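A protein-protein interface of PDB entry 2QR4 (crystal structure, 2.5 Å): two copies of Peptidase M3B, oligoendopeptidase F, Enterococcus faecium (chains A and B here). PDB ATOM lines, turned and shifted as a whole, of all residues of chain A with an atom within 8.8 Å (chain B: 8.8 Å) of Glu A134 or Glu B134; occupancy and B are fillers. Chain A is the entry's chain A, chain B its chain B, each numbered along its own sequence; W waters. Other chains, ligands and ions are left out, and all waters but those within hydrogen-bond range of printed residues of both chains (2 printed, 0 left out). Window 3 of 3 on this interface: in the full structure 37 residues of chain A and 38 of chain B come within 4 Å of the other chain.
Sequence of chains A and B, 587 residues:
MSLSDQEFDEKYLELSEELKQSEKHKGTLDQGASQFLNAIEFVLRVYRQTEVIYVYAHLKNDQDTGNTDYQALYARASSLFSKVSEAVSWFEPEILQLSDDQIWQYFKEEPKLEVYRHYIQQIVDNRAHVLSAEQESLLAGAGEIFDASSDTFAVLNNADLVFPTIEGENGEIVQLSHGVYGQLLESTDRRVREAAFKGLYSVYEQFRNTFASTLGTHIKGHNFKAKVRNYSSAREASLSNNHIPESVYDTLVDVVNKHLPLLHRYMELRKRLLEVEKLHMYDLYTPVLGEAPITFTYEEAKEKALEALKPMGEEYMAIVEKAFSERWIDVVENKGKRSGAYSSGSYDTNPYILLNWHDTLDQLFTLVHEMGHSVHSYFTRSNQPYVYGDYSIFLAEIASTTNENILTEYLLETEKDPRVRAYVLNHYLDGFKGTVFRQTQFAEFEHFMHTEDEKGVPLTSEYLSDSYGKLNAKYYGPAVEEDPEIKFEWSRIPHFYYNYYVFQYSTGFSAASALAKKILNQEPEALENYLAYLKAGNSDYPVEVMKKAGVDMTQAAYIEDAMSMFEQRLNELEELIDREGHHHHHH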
ATOM      1  N   LYS A  26      10.901  37.163  28.940  1.00  0.00           N
ATOM      2  CA  LYS A  26      10.844  36.251  27.815  1.00  0.00           C
ATOM      3  C   LYS A  26       9.627  36.554  26.951  1.00  0.00           C
ATOM      4  O   LYS A  26       8.534  36.777  27.460  1.00  0.00           O
ATOM      5  CB  LYS A  26      10.825  34.801  28.310  1.00  0.00           C
ATOM      6  CG  LYS A  26      10.721  33.761  27.221  1.00  0.00           C
ATOM      7  CD  LYS A  26      10.946  32.352  27.757  1.00  0.00           C
ATOM      8  CE  LYS A  26      10.691  31.321  26.661  1.00  0.00           C
ATOM      9  NZ  LYS A  26      11.009  29.941  27.100  1.00  0.00           N
ATOM     10  N   GLU A  86      21.018  28.617  31.754  1.00  0.00           N
ATOM     11  CA  GLU A  86      19.893  27.949  31.149  1.00  0.00           C
ATOM     12  C   GLU A  86      18.660  28.855  31.155  1.00  0.00           C
ATOM     13  O   GLU A  86      17.943  28.958  30.152  1.00  0.00           O
ATOM     14  CB  GLU A  86      19.595  26.624  31.863  1.00  0.00           C
ATOM     15  CG  GLU A  86      18.593  25.736  31.114  1.00  0.00           C
ATOM     16  CD  GLU A  86      17.161  26.254  31.211  1.00  0.00           C
ATOM     17  OE1 GLU A  86      16.836  26.924  32.220  1.00  0.00           O
ATOM     18  OE2 GLU A  86      16.359  25.992  30.283  1.00  0.00           O
ATOM     19  N   SER A  89      18.813  31.545  28.486  1.00  0.00           N
ATOM     20  CA  SER A  89      19.208  31.075  27.160  1.00  0.00           C
ATOM     21  C   SER A  89      18.228  31.435  26.035  1.00  0.00           C
ATOM     22  O   SER A  89      18.567  31.302  24.864  1.00  0.00           O
ATOM     23  CB  SER A  89      19.437  29.554  27.181  1.00  0.00           C
ATOM     24  OG  SER A  89      18.245  28.852  27.522  1.00  0.00           O
ATOM     25  N   TRP A  90      17.017  31.872  26.380  1.00  0.00           N
ATOM     26  CA  TRP A  90      16.042  32.272  25.360  1.00  0.00           C
ATOM     27  C   TRP A  90      16.419  33.625  24.746  1.00  0.00           C
ATOM     28  O   TRP A  90      15.941  33.999  23.673  1.00  0.00           O
ATOM     29  CB  TRP A  90      14.650  32.364  25.971  1.00  0.00           C
ATOM     30  CG  TRP A  90      14.639  33.272  27.158  1.00  0.00           C
ATOM     31  CD1 TRP A  90      14.770  32.911  28.469  1.00  0.00           C
ATOM     32  CD2 TRP A  90      14.517  34.694  27.142  1.00  0.00           C
ATOM     33  NE1 TRP A  90      14.727  34.015  29.268  1.00  0.00           N
ATOM     34  CE2 TRP A  90      14.579  35.130  28.481  1.00  0.00           C
ATOM     35  CE3 TRP A  90      14.353  35.647  26.122  1.00  0.00           C
ATOM     36  CZ2 TRP A  90      14.505  36.481  28.837  1.00  0.00           C
ATOM     37  CZ3 TRP A  90      14.273  36.983  26.472  1.00  0.00           C
ATOM     38  CH2 TRP A  90      14.350  37.390  27.824  1.00  0.00           C
ATOM     39  N   PRO A  93      18.483  34.009  20.975  1.00  0.00           N
ATOM     40  CA  PRO A  93      17.508  33.556  19.988  1.00  0.00           C
ATOM     41  C   PRO A  93      16.362  34.545  19.815  1.00  0.00           C
ATOM     42  O   PRO A  93      15.954  34.809  18.683  1.00  0.00           O
ATOM     43  CB  PRO A  93      16.999  32.236  20.581  1.00  0.00           C
ATOM     44  CG  PRO A  93      18.206  31.727  21.351  1.00  0.00           C
ATOM     45  CD  PRO A  93      18.817  32.959  21.952  1.00  0.00           C
ATOM     46  N   VAL A 130      24.232  31.373  16.570  1.00  0.00           N
ATOM     47  CA  VAL A 130      23.262  31.276  17.648  1.00  0.00           C
ATOM     48  C   VAL A 130      22.134  30.351  17.209  1.00  0.00           C
ATOM     49  O   VAL A 130      21.716  30.383  16.058  1.00  0.00           O
ATOM     50  CB  VAL A 130      22.695  32.645  18.035  1.00  0.00           C
ATOM     51  CG1 VAL A 130      21.651  32.490  19.126  1.00  0.00           C
ATOM     52  CG2 VAL A 130      23.815  33.563  18.485  1.00  0.00           C
ATOM     53  N   LEU A 131      21.648  29.528  18.129  1.00  0.00           N
ATOM     54  CA  LEU A 131      20.713  28.464  17.786  1.00  0.00           C
ATOM     55  C   LEU A 131      19.312  28.842  18.251  1.00  0.00           C
ATOM     56  O   LEU A 131      19.051  29.999  18.549  1.00  0.00           O
ATOM     57  CB  LEU A 131      21.178  27.130  18.389  1.00  0.00           C
ATOM     58  CG  LEU A 131      22.526  26.630  17.841  1.00  0.00           C
ATOM     59  CD1 LEU A 131      22.994  25.376  18.539  1.00  0.00           C
ATOM     60  CD2 LEU A 131      22.468  26.382  16.340  1.00  0.00           C
ATOM     61  N   SER A 132      18.393  27.887  18.276  1.00  0.00           N
ATOM     62  CA  SER A 132      17.049  28.182  18.756  1.00  0.00           C
ATOM     63  C   SER A 132      17.050  28.172  20.284  1.00  0.00           C
ATOM     64  O   SER A 132      18.008  27.716  20.908  1.00  0.00           O
ATOM     65  CB  SER A 132      16.056  27.156  18.214  1.00  0.00           C
ATOM     66  OG  SER A 132      16.325  25.875  18.748  1.00  0.00           O
ATOM     67  N   ALA A 133      15.975  28.652  20.885  1.00  0.00           N
ATOM     68  CA  ALA A 133      15.861  28.638  22.339  1.00  0.00           C
ATOM     69  C   ALA A 133      15.985  27.219  22.870  1.00  0.00           C
ATOM     70  O   ALA A 133      16.678  26.991  23.857  1.00  0.00           O
ATOM     71  CB  ALA A 133      14.544  29.263  22.778  1.00  0.00           C
ATOM     72  N   GLU A 134      15.334  26.266  22.203  1.00  0.00           N
ATOM     73  CA  GLU A 134      15.386  24.848  22.612  1.00  0.00           C
ATOM     74  C   GLU A 134      16.820  24.313  22.668  1.00  0.00           C
ATOM     75  O   GLU A 134      17.202  23.647  23.624  1.00  0.00           O
ATOM     76  CB  GLU A 134      14.576  23.952  21.663  1.00  0.00           C
ATOM     77  CG  GLU A 134      13.080  23.845  21.926  1.00  0.00           C
ATOM     78  CD  GLU A 134      12.404  22.714  21.091  1.00  0.00           C
ATOM     79  OE1 GLU A 134      11.202  22.450  21.327  1.00  0.00           O
ATOM     80  OE2 GLU A 134      13.055  22.089  20.204  1.00  0.00           O
ATOM     81  N   GLN A 135      17.597  24.582  21.624  1.00  0.00           N
ATOM     82  CA  GLN A 135      18.963  24.083  21.553  1.00  0.00           C
ATOM     83  C   GLN A 135      19.867  24.788  22.547  1.00  0.00           C
ATOM     84  O   GLN A 135      20.641  24.134  23.228  1.00  0.00           O
ATOM     85  CB  GLN A 135      19.525  24.224  20.141  1.00  0.00           C
ATOM     86  CG  GLN A 135      18.744  23.469  19.075  1.00  0.00           C
ATOM     87  CD  GLN A 135      19.050  23.962  17.667  1.00  0.00           C
ATOM     88  OE1 GLN A 135      18.825  25.132  17.348  1.00  0.00           O
ATOM     89  NE2 GLN A 135      19.554  23.068  16.816  1.00  0.00           N
ATOM     90  N   GLU A 136      19.778  26.116  22.625  1.00  0.00           N
ATOM     91  CA  GLU A 136      20.597  26.899  23.565  1.00  0.00           C
ATOM     92  C   GLU A 136      20.330  26.441  24.994  1.00  0.00           C
ATOM     93  O   GLU A 136      21.254  26.337  25.813  1.00  0.00           O
ATOM     94  CB  GLU A 136      20.324  28.420  23.452  1.00  0.00           C
ATOM     95  CG  GLU A 136      20.798  29.044  22.152  1.00  0.00           C
ATOM     96  CD  GLU A 136      22.312  28.964  21.979  1.00  0.00           C
ATOM     97  OE1 GLU A 136      22.999  28.623  22.972  1.00  0.00           O
ATOM     98  OE2 GLU A 136      22.820  29.248  20.860  1.00  0.00           O
ATOM     99  N   SER A 137      19.062  26.168  25.287  1.00  0.00           N
ATOM    100  CA  SER A 137      18.682  25.606  26.579  1.00  0.00           C
ATOM    101  C   SER A 137      19.400  24.276  26.897  1.00  0.00           C
ATOM    102  O   SER A 137      19.961  24.111  27.986  1.00  0.00           O
ATOM    103  CB  SER A 137      17.169  25.454  26.669  1.00  0.00           C
ATOM    104  OG  SER A 137      16.810  24.920  27.920  1.00  0.00           O
ATOM    105  N   LEU A 138      19.421  23.343  25.948  1.00  0.00           N
ATOM    106  CA  LEU A 138      20.156  22.081  26.160  1.00  0.00           C
ATOM    107  C   LEU A 138      21.644  22.292  26.394  1.00  0.00           C
ATOM    108  O   LEU A 138      22.227  21.729  27.326  1.00  0.00           O
ATOM    109  CB  LEU A 138      19.987  21.147  24.969  1.00  0.00           C
ATOM    110  CG  LEU A 138      19.100  19.921  25.122  1.00  0.00           C
ATOM    111  CD1 LEU A 138      18.159  20.052  26.292  1.00  0.00           C
ATOM    112  CD2 LEU A 138      18.352  19.740  23.839  1.00  0.00           C
ATOM    113  N   LEU A 139      22.260  23.084  25.523  1.00  0.00           N
ATOM    114  CA  LEU A 139      23.685  23.372  25.601  1.00  0.00           C
ATOM    115  C   LEU A 139      24.073  24.062  26.911  1.00  0.00           C
ATOM    116  O   LEU A 139      25.093  23.720  27.505  1.00  0.00           O
ATOM    117  CB  LEU A 139      24.120  24.235  24.411  1.00  0.00           C
ATOM    118  CG  LEU A 139      24.759  23.591  23.173  1.00  0.00           C
ATOM    119  CD1 LEU A 139      24.582  22.094  23.148  1.00  0.00           C
ATOM    120  CD2 LEU A 139      24.217  24.225  21.898  1.00  0.00           C
ATOM    121  N   ALA A 140      23.271  25.031  27.356  1.00  0.00           N
ATOM    122  CA  ALA A 140      23.600  25.759  28.576  1.00  0.00           C
ATOM    123  C   ALA A 140      23.472  24.827  29.753  1.00  0.00           C
ATOM    124  O   ALA A 140      24.368  24.750  30.598  1.00  0.00           O
ATOM    125  CB  ALA A 140      22.693  26.977  28.768  1.00  0.00           C
ATOM    126  N   GLY A 141      22.355  24.110  29.795  1.00  0.00           N
ATOM    127  CA  GLY A 141      22.077  23.207  30.901  1.00  0.00           C
ATOM    128  C   GLY A 141      23.057  22.048  31.014  1.00  0.00           C
ATOM    129  O   GLY A 141      23.177  21.439  32.074  1.00  0.00           O
ATOM    130  N   PHE A 224      32.384  19.259  19.079  1.00  0.00           N
ATOM    131  CA  PHE A 224      30.950  19.111  19.042  1.00  0.00           C
ATOM    132  C   PHE A 224      30.247  20.483  19.023  1.00  0.00           C
ATOM    133  O   PHE A 224      29.325  20.688  18.227  1.00  0.00           O
ATOM    134  CB  PHE A 224      30.470  18.290  20.237  1.00  0.00           C
ATOM    135  CG  PHE A 224      28.977  18.296  20.396  1.00  0.00           C
ATOM    136  CD1 PHE A 224      28.182  17.529  19.566  1.00  0.00           C
ATOM    137  CD2 PHE A 224      28.371  19.104  21.337  1.00  0.00           C
ATOM    138  CE1 PHE A 224      26.806  17.553  19.682  1.00  0.00           C
ATOM    139  CE2 PHE A 224      26.991  19.139  21.463  1.00  0.00           C
ATOM    140  CZ  PHE A 224      26.210  18.352  20.643  1.00  0.00           C
ATOM    141  N   VAL A 228      27.878  22.001  15.972  1.00  0.00           N
ATOM    142  CA  VAL A 228      26.447  22.299  16.060  1.00  0.00           C
ATOM    143  C   VAL A 228      26.144  23.790  15.946  1.00  0.00           C
ATOM    144  O   VAL A 228      25.007  24.162  15.679  1.00  0.00           O
ATOM    145  CB  VAL A 228      25.770  21.666  17.303  1.00  0.00           C
ATOM    146  CG1 VAL A 228      26.062  20.174  17.327  1.00  0.00           C
ATOM    147  CG2 VAL A 228      26.241  22.340  18.598  1.00  0.00           C
ATOM    148  N   LYS B  26      14.095  10.163   6.217  1.00  0.00           N
ATOM    149  CA  LYS B  26      13.613  11.286   6.996  1.00  0.00           C
ATOM    150  C   LYS B  26      12.451  11.977   6.294  1.00  0.00           C
ATOM    151  O   LYS B  26      12.525  12.281   5.105  1.00  0.00           O
ATOM    152  CB  LYS B  26      14.754  12.281   7.233  1.00  0.00           C
ATOM    153  CG  LYS B  26      14.390  13.433   8.157  1.00  0.00           C
ATOM    154  CD  LYS B  26      15.614  14.270   8.506  1.00  0.00           C
ATOM    155  CE  LYS B  26      15.262  15.444   9.415  1.00  0.00           C
ATOM    156  NZ  LYS B  26      16.492  16.135   9.899  1.00  0.00           N
ATOM    157  N   GLU B  86      22.885  10.023  16.090  1.00  0.00           N
ATOM    158  CA  GLU B  86      22.482  11.355  15.666  1.00  0.00           C
ATOM    159  C   GLU B  86      21.752  11.324  14.323  1.00  0.00           C
ATOM    160  O   GLU B  86      20.732  11.976  14.167  1.00  0.00           O
ATOM    161  CB  GLU B  86      23.687  12.297  15.605  1.00  0.00           C
ATOM    162  CG  GLU B  86      23.310  13.768  15.542  1.00  0.00           C
ATOM    163  CD  GLU B  86      22.836  14.193  14.165  1.00  0.00           C
ATOM    164  OE1 GLU B  86      23.406  13.724  13.167  1.00  0.00           O
ATOM    165  OE2 GLU B  86      21.889  15.002  14.073  1.00  0.00           O
ATOM    166  N   SER B  89      18.239  10.188  14.820  1.00  0.00           N
ATOM    167  CA  SER B  89      17.543  10.825  15.931  1.00  0.00           C
ATOM    168  C   SER B  89      16.214  11.456  15.526  1.00  0.00           C
ATOM    169  O   SER B  89      15.427  11.805  16.384  1.00  0.00           O
ATOM    170  CB  SER B  89      18.439  11.894  16.567  1.00  0.00           C
ATOM    171  OG  SER B  89      18.704  12.950  15.658  1.00  0.00           O
ATOM    172  N   TRP B  90      15.966  11.612  14.227  1.00  0.00           N
ATOM    173  CA  TRP B  90      14.702  12.181  13.755  1.00  0.00           C
ATOM    174  C   TRP B  90      13.560  11.173  13.863  1.00  0.00           C
ATOM    175  O   TRP B  90      12.382  11.549  13.869  1.00  0.00           O
ATOM    176  CB  TRP B  90      14.818  12.649  12.303  1.00  0.00           C
ATOM    177  CG  TRP B  90      15.321  11.578  11.405  1.00  0.00           C
ATOM    178  CD1 TRP B  90      16.619  11.356  11.043  1.00  0.00           C
ATOM    179  CD2 TRP B  90      14.544  10.554  10.767  1.00  0.00           C
ATOM    180  NE1 TRP B  90      16.697  10.264  10.207  1.00  0.00           N
ATOM    181  CE2 TRP B  90      15.440   9.751  10.028  1.00  0.00           C
ATOM    182  CE3 TRP B  90      13.182  10.248  10.733  1.00  0.00           C
ATOM    183  CZ2 TRP B  90      15.017   8.668   9.274  1.00  0.00           C
ATOM    184  CZ3 TRP B  90      12.764   9.166   9.980  1.00  0.00           C
ATOM    185  CH2 TRP B  90      13.680   8.389   9.264  1.00  0.00           C
ATOM    186  N   PRO B  93      10.817  11.172  17.070  1.00  0.00           N
ATOM    187  CA  PRO B  93       9.947  12.354  17.027  1.00  0.00           C
ATOM    188  C   PRO B  93       9.011  12.331  15.823  1.00  0.00           C
ATOM    189  O   PRO B  93       7.871  12.765  15.928  1.00  0.00           O
ATOM    190  CB  PRO B  93      10.936  13.532  16.930  1.00  0.00           C
ATOM    191  CG  PRO B  93      12.238  12.989  17.487  1.00  0.00           C
ATOM    192  CD  PRO B  93      12.251  11.533  17.072  1.00  0.00           C
ATOM    193  N   GLN B  97       4.779  12.278  15.525  1.00  0.00           N
ATOM    194  CA  GLN B  97       4.017  13.357  14.882  1.00  0.00           C
ATOM    195  C   GLN B  97       2.745  12.755  14.303  1.00  0.00           C
ATOM    196  O   GLN B  97       1.793  13.457  13.981  1.00  0.00           O
ATOM    197  CB  GLN B  97       4.830  14.034  13.798  1.00  0.00           C
ATOM    198  CG  GLN B  97       5.736  15.145  14.314  1.00  0.00           C
ATOM    199  CD  GLN B  97       6.697  15.631  13.243  1.00  0.00           C
ATOM    200  OE1 GLN B  97       6.662  15.171  12.102  1.00  0.00           O
ATOM    201  NE2 GLN B  97       7.568  16.544  13.610  1.00  0.00           N
ATOM    202  N   LEU B 131      11.676  13.982  22.828  1.00  0.00           N
ATOM    203  CA  LEU B 131      11.715  15.415  22.561  1.00  0.00           C
ATOM    204  C   LEU B 131      11.604  15.701  21.065  1.00  0.00           C
ATOM    205  O   LEU B 131      11.283  14.817  20.272  1.00  0.00           O
ATOM    206  CB  LEU B 131      13.022  15.975  23.126  1.00  0.00           C
ATOM    207  CG  LEU B 131      13.182  15.656  24.615  1.00  0.00           C
ATOM    208  CD1 LEU B 131      14.580  16.033  25.118  1.00  0.00           C
ATOM    209  CD2 LEU B 131      12.084  16.378  25.416  1.00  0.00           C
ATOM    210  N   SER B 132      11.889  16.930  20.669  1.00  0.00           N
ATOM    211  CA  SER B 132      11.861  17.270  19.257  1.00  0.00           C
ATOM    212  C   SER B 132      13.094  16.721  18.536  1.00  0.00           C
ATOM    213  O   SER B 132      14.049  16.264  19.165  1.00  0.00           O
ATOM    214  CB  SER B 132      11.769  18.787  19.077  1.00  0.00           C
ATOM    215  OG  SER B 132      13.067  19.379  19.120  1.00  0.00           O
ATOM    216  N   ALA B 133      13.052  16.786  17.209  1.00  0.00           N
ATOM    217  CA  ALA B 133      14.151  16.393  16.328  1.00  0.00           C
ATOM    218  C   ALA B 133      15.457  17.136  16.653  1.00  0.00           C
ATOM    219  O   ALA B 133      16.520  16.531  16.727  1.00  0.00           O
ATOM    220  CB  ALA B 133      13.737  16.649  14.832  1.00  0.00           C
ATOM    221  N   GLU B 134      15.353  18.452  16.837  1.00  0.00           N
ATOM    222  CA  GLU B 134      16.488  19.307  17.150  1.00  0.00           C
ATOM    223  C   GLU B 134      17.092  18.878  18.477  1.00  0.00           C
ATOM    224  O   GLU B 134      18.310  18.759  18.594  1.00  0.00           O
ATOM    225  CB  GLU B 134      16.068  20.777  17.264  1.00  0.00           C
ATOM    226  CG  GLU B 134      15.734  21.516  15.984  1.00  0.00           C
ATOM    227  CD  GLU B 134      15.595  23.060  16.208  1.00  0.00           C
ATOM    228  OE1 GLU B 134      15.955  23.826  15.281  1.00  0.00           O
ATOM    229  OE2 GLU B 134      15.130  23.518  17.296  1.00  0.00           O
ATOM    230  N   GLN B 135      16.241  18.651  19.476  1.00  0.00           N
ATOM    231  CA  GLN B 135      16.722  18.264  20.815  1.00  0.00           C
ATOM    232  C   GLN B 135      17.314  16.864  20.820  1.00  0.00           C
ATOM    233  O   GLN B 135      18.343  16.636  21.441  1.00  0.00           O
ATOM    234  CB  GLN B 135      15.588  18.321  21.834  1.00  0.00           C
ATOM    235  CG  GLN B 135      15.135  19.718  22.208  1.00  0.00           C
ATOM    236  CD  GLN B 135      13.736  19.729  22.806  1.00  0.00           C
ATOM    237  OE1 GLN B 135      12.836  19.037  22.318  1.00  0.00           O
ATOM    238  NE2 GLN B 135      13.544  20.519  23.863  1.00  0.00           N
ATOM    239  N   GLU B 136      16.672  15.920  20.127  1.00  0.00           N
ATOM    240  CA  GLU B 136      17.193  14.552  20.106  1.00  0.00           C
ATOM    241  C   GLU B 136      18.518  14.507  19.369  1.00  0.00           C
ATOM    242  O   GLU B 136      19.416  13.756  19.743  1.00  0.00           O
ATOM    243  CB  GLU B 136      16.200  13.543  19.493  1.00  0.00           C
ATOM    244  CG  GLU B 136      14.916  13.356  20.310  1.00  0.00           C
ATOM    245  CD  GLU B 136      15.123  12.597  21.620  1.00  0.00           C
ATOM    246  OE1 GLU B 136      16.261  12.159  21.902  1.00  0.00           O
ATOM    247  OE2 GLU B 136      14.139  12.442  22.377  1.00  0.00           O
ATOM    248  N   SER B 137      18.645  15.330  18.334  1.00  0.00           N
ATOM    249  CA  SER B 137      19.878  15.378  17.564  1.00  0.00           C
ATOM    250  C   SER B 137      21.030  15.897  18.450  1.00  0.00           C
ATOM    251  O   SER B 137      22.146  15.369  18.444  1.00  0.00           O
ATOM    252  CB  SER B 137      19.684  16.268  16.330  1.00  0.00           C
ATOM    253  OG  SER B 137      20.932  16.723  15.835  1.00  0.00           O
ATOM    254  N   LEU B 138      20.747  16.919  19.237  1.00  0.00           N
ATOM    255  CA  LEU B 138      21.770  17.491  20.093  1.00  0.00           C
ATOM    256  C   LEU B 138      22.169  16.480  21.175  1.00  0.00           C
ATOM    257  O   LEU B 138      23.355  16.248  21.415  1.00  0.00           O
ATOM    258  CB  LEU B 138      21.250  18.781  20.703  1.00  0.00           C
ATOM    259  CG  LEU B 138      22.129  20.015  20.829  1.00  0.00           C
ATOM    260  CD1 LEU B 138      22.937  20.288  19.577  1.00  0.00           C
ATOM    261  CD2 LEU B 138      21.174  21.137  21.066  1.00  0.00           C
ATOM    262  N   LEU B 139      21.178  15.852  21.802  1.00  0.00           N
ATOM    263  CA  LEU B 139      21.444  14.886  22.872  1.00  0.00           C
ATOM    264  C   LEU B 139      22.231  13.677  22.362  1.00  0.00           C
ATOM    265  O   LEU B 139      23.177  13.230  23.006  1.00  0.00           O
ATOM    266  CB  LEU B 139      20.141  14.437  23.543  1.00  0.00           C
ATOM    267  CG  LEU B 139      19.729  14.986  24.919  1.00  0.00           C
ATOM    268  CD1 LEU B 139      20.432  16.268  25.246  1.00  0.00           C
ATOM    269  CD2 LEU B 139      18.221  15.168  24.999  1.00  0.00           C
ATOM    270  N   ALA B 140      21.855  13.156  21.198  1.00  0.00           N
ATOM    271  CA  ALA B 140      22.527  11.977  20.661  1.00  0.00           C
ATOM    272  C   ALA B 140      23.963  12.300  20.229  1.00  0.00           C
ATOM    273  O   ALA B 140      24.874  11.497  20.426  1.00  0.00           O
ATOM    274  CB  ALA B 140      21.714  11.362  19.481  1.00  0.00           C
ATOM    275  N   GLY B 141      24.165  13.477  19.642  1.00  0.00           N
ATOM    276  CA  GLY B 141      25.496  13.889  19.208  1.00  0.00           C
ATOM    277  C   GLY B 141      26.476  14.097  20.356  1.00  0.00           C
ATOM    278  O   GLY B 141      27.675  13.979  20.179  1.00  0.00           O
ATOM    279  N   PHE B 224      20.447  15.214  34.647  1.00  0.00           N
ATOM    280  CA  PHE B 224      20.182  16.187  33.602  1.00  0.00           C
ATOM    281  C   PHE B 224      19.303  15.596  32.524  1.00  0.00           C
ATOM    282  O   PHE B 224      18.359  16.242  32.067  1.00  0.00           O
ATOM    283  CB  PHE B 224      21.483  16.682  32.990  1.00  0.00           C
ATOM    284  CG  PHE B 224      21.294  17.443  31.719  1.00  0.00           C
ATOM    285  CD1 PHE B 224      20.880  18.758  31.747  1.00  0.00           C
ATOM    286  CD2 PHE B 224      21.548  16.844  30.490  1.00  0.00           C
ATOM    287  CE1 PHE B 224      20.710  19.470  30.568  1.00  0.00           C
ATOM    288  CE2 PHE B 224      21.390  17.553  29.314  1.00  0.00           C
ATOM    289  CZ  PHE B 224      20.962  18.869  29.357  1.00  0.00           C
ATOM    290  N   VAL B 228      15.365  16.894  31.407  1.00  0.00           N
ATOM    291  CA  VAL B 228      14.945  17.399  30.092  1.00  0.00           C
ATOM    292  C   VAL B 228      13.920  16.482  29.441  1.00  0.00           C
ATOM    293  O   VAL B 228      13.092  16.929  28.661  1.00  0.00           O
ATOM    294  CB  VAL B 228      16.129  17.716  29.136  1.00  0.00           C
ATOM    295  CG1 VAL B 228      17.037  18.768  29.778  1.00  0.00           C
ATOM    296  CG2 VAL B 228      16.923  16.432  28.741  1.00  0.00           C
HETATM  297  O   HOH W   1      15.181  22.234  25.014  1.00  0.00           O
HETATM  298  O   HOH W   2      19.949  20.321  17.242  1.00  0.00           O
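N of Ser B132 sits at hydrogen-bond distance from OE1 of Gln B135, at 2.8 Å. The side-chain hydroxyl (OG) of Ser B132 lies close to the backbone NH (N) of Glu B134 (3.4 Å). The backbone NH of Ser A132 sits at hydrogen-bond distance from the side-chain amide oxygen of Gln A135, at 2.9 Å.
Glu B134 touches its own counterpart, Glu A134. Glu A134 touches Gln B135, and with the chains exchanged Gln A135 touches Glu B134. Leu A138 touches Leu B139, and with the chains exchanged Leu A139 touches Leu B138. Leu A138 touches Phe B224, and with the chains exchanged Phe A224 touches Leu B138. 18 positions are printed for both chains.
Among the printed residues, merely in contact across the chains: Gly A141 with Phe B224 (3.5 Å), Phe A224 with Gly B141 (3.5 Å), Glu A134 with Gln B135 (3.6 Å), Leu A138 with Gln B135 (3.6 Å), Gln A135 with Leu B138 (3.6 Å), Phe A224 with Leu B138 (3.6 Å), Leu A138 with Phe B224 (3.7 Å), Gln A135 with Glu B134 (3.8 Å), Glu A134 with Glu B134 (3.8 Å), Val A228 with Leu B138 (3.9 Å), Leu A138 with Val B228 (3.9 Å), Leu A138 with Leu B139 (3.9 Å) and Leu A139 with Leu B138 (3.96 Å).
Hydrophobic or aromatic side chains of chain A within 4 Å of the printed part of chain B: Leu A138, Leu A139, Phe A224 and Val A228. Among the printed residues, 15 pairs touch across the chains. Among the printed residues, no Asp or Glu carboxylate lies within 4 Å of a Lys or Arg side-chain nitrogen of the other chain.
The side-chain carboxylate (OE2) of Glu B134 is in hydrogen-bond range of the side-chain hydroxyl (OG) of Ser A132 (3.0 Å). The side-chain hydroxyl of Ser B132 sits at hydrogen-bond distance from the side-chain carboxylate of Glu A134 (2.9 Å).
Of the printed residues of chain B, Ser A132 touches Glu B134. No residue of chain B comes within 4 Å of Ala A133. Of the printed residues of chain B, Phe A224 touches Leu B138 (3.6 Å) and Gly B141 (3.5 Å). Printed residues of chain B within 4 Å of Val A228: Leu B138 (3.9 Å). No residue of chain A comes within 4 Å of Ala B133. Glu B134 touches three residues of chain A. Gln B135 touches just these residues of chain A: Glu A134 (3.6 Å) and Leu A138 (3.6 Å). Ser B137 touches none of the printed residues of chain A. Ala B140 touches none of the printed residues of chain A. The nearest residue of chain B that does not touch Glu A134 is Leu B138 (5.3 Å). The nearest printed residue of chain A that does not touch Val B228 is Ser A137 (6.3 Å).
Water W1 lies within hydrogen-bond range of the side-chain amide nitrogen (NE2) of Gln B135 (2.6 Å) and the backbone carbonyl oxygen (O) of Glu A134 (2.8 Å). Water W2 bridges the backbone carbonyl oxygen (O) of Glu B134 (2.6 Å) and the side-chain amide nitrogen (NE2) of Gln A135 (2.8 Å).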
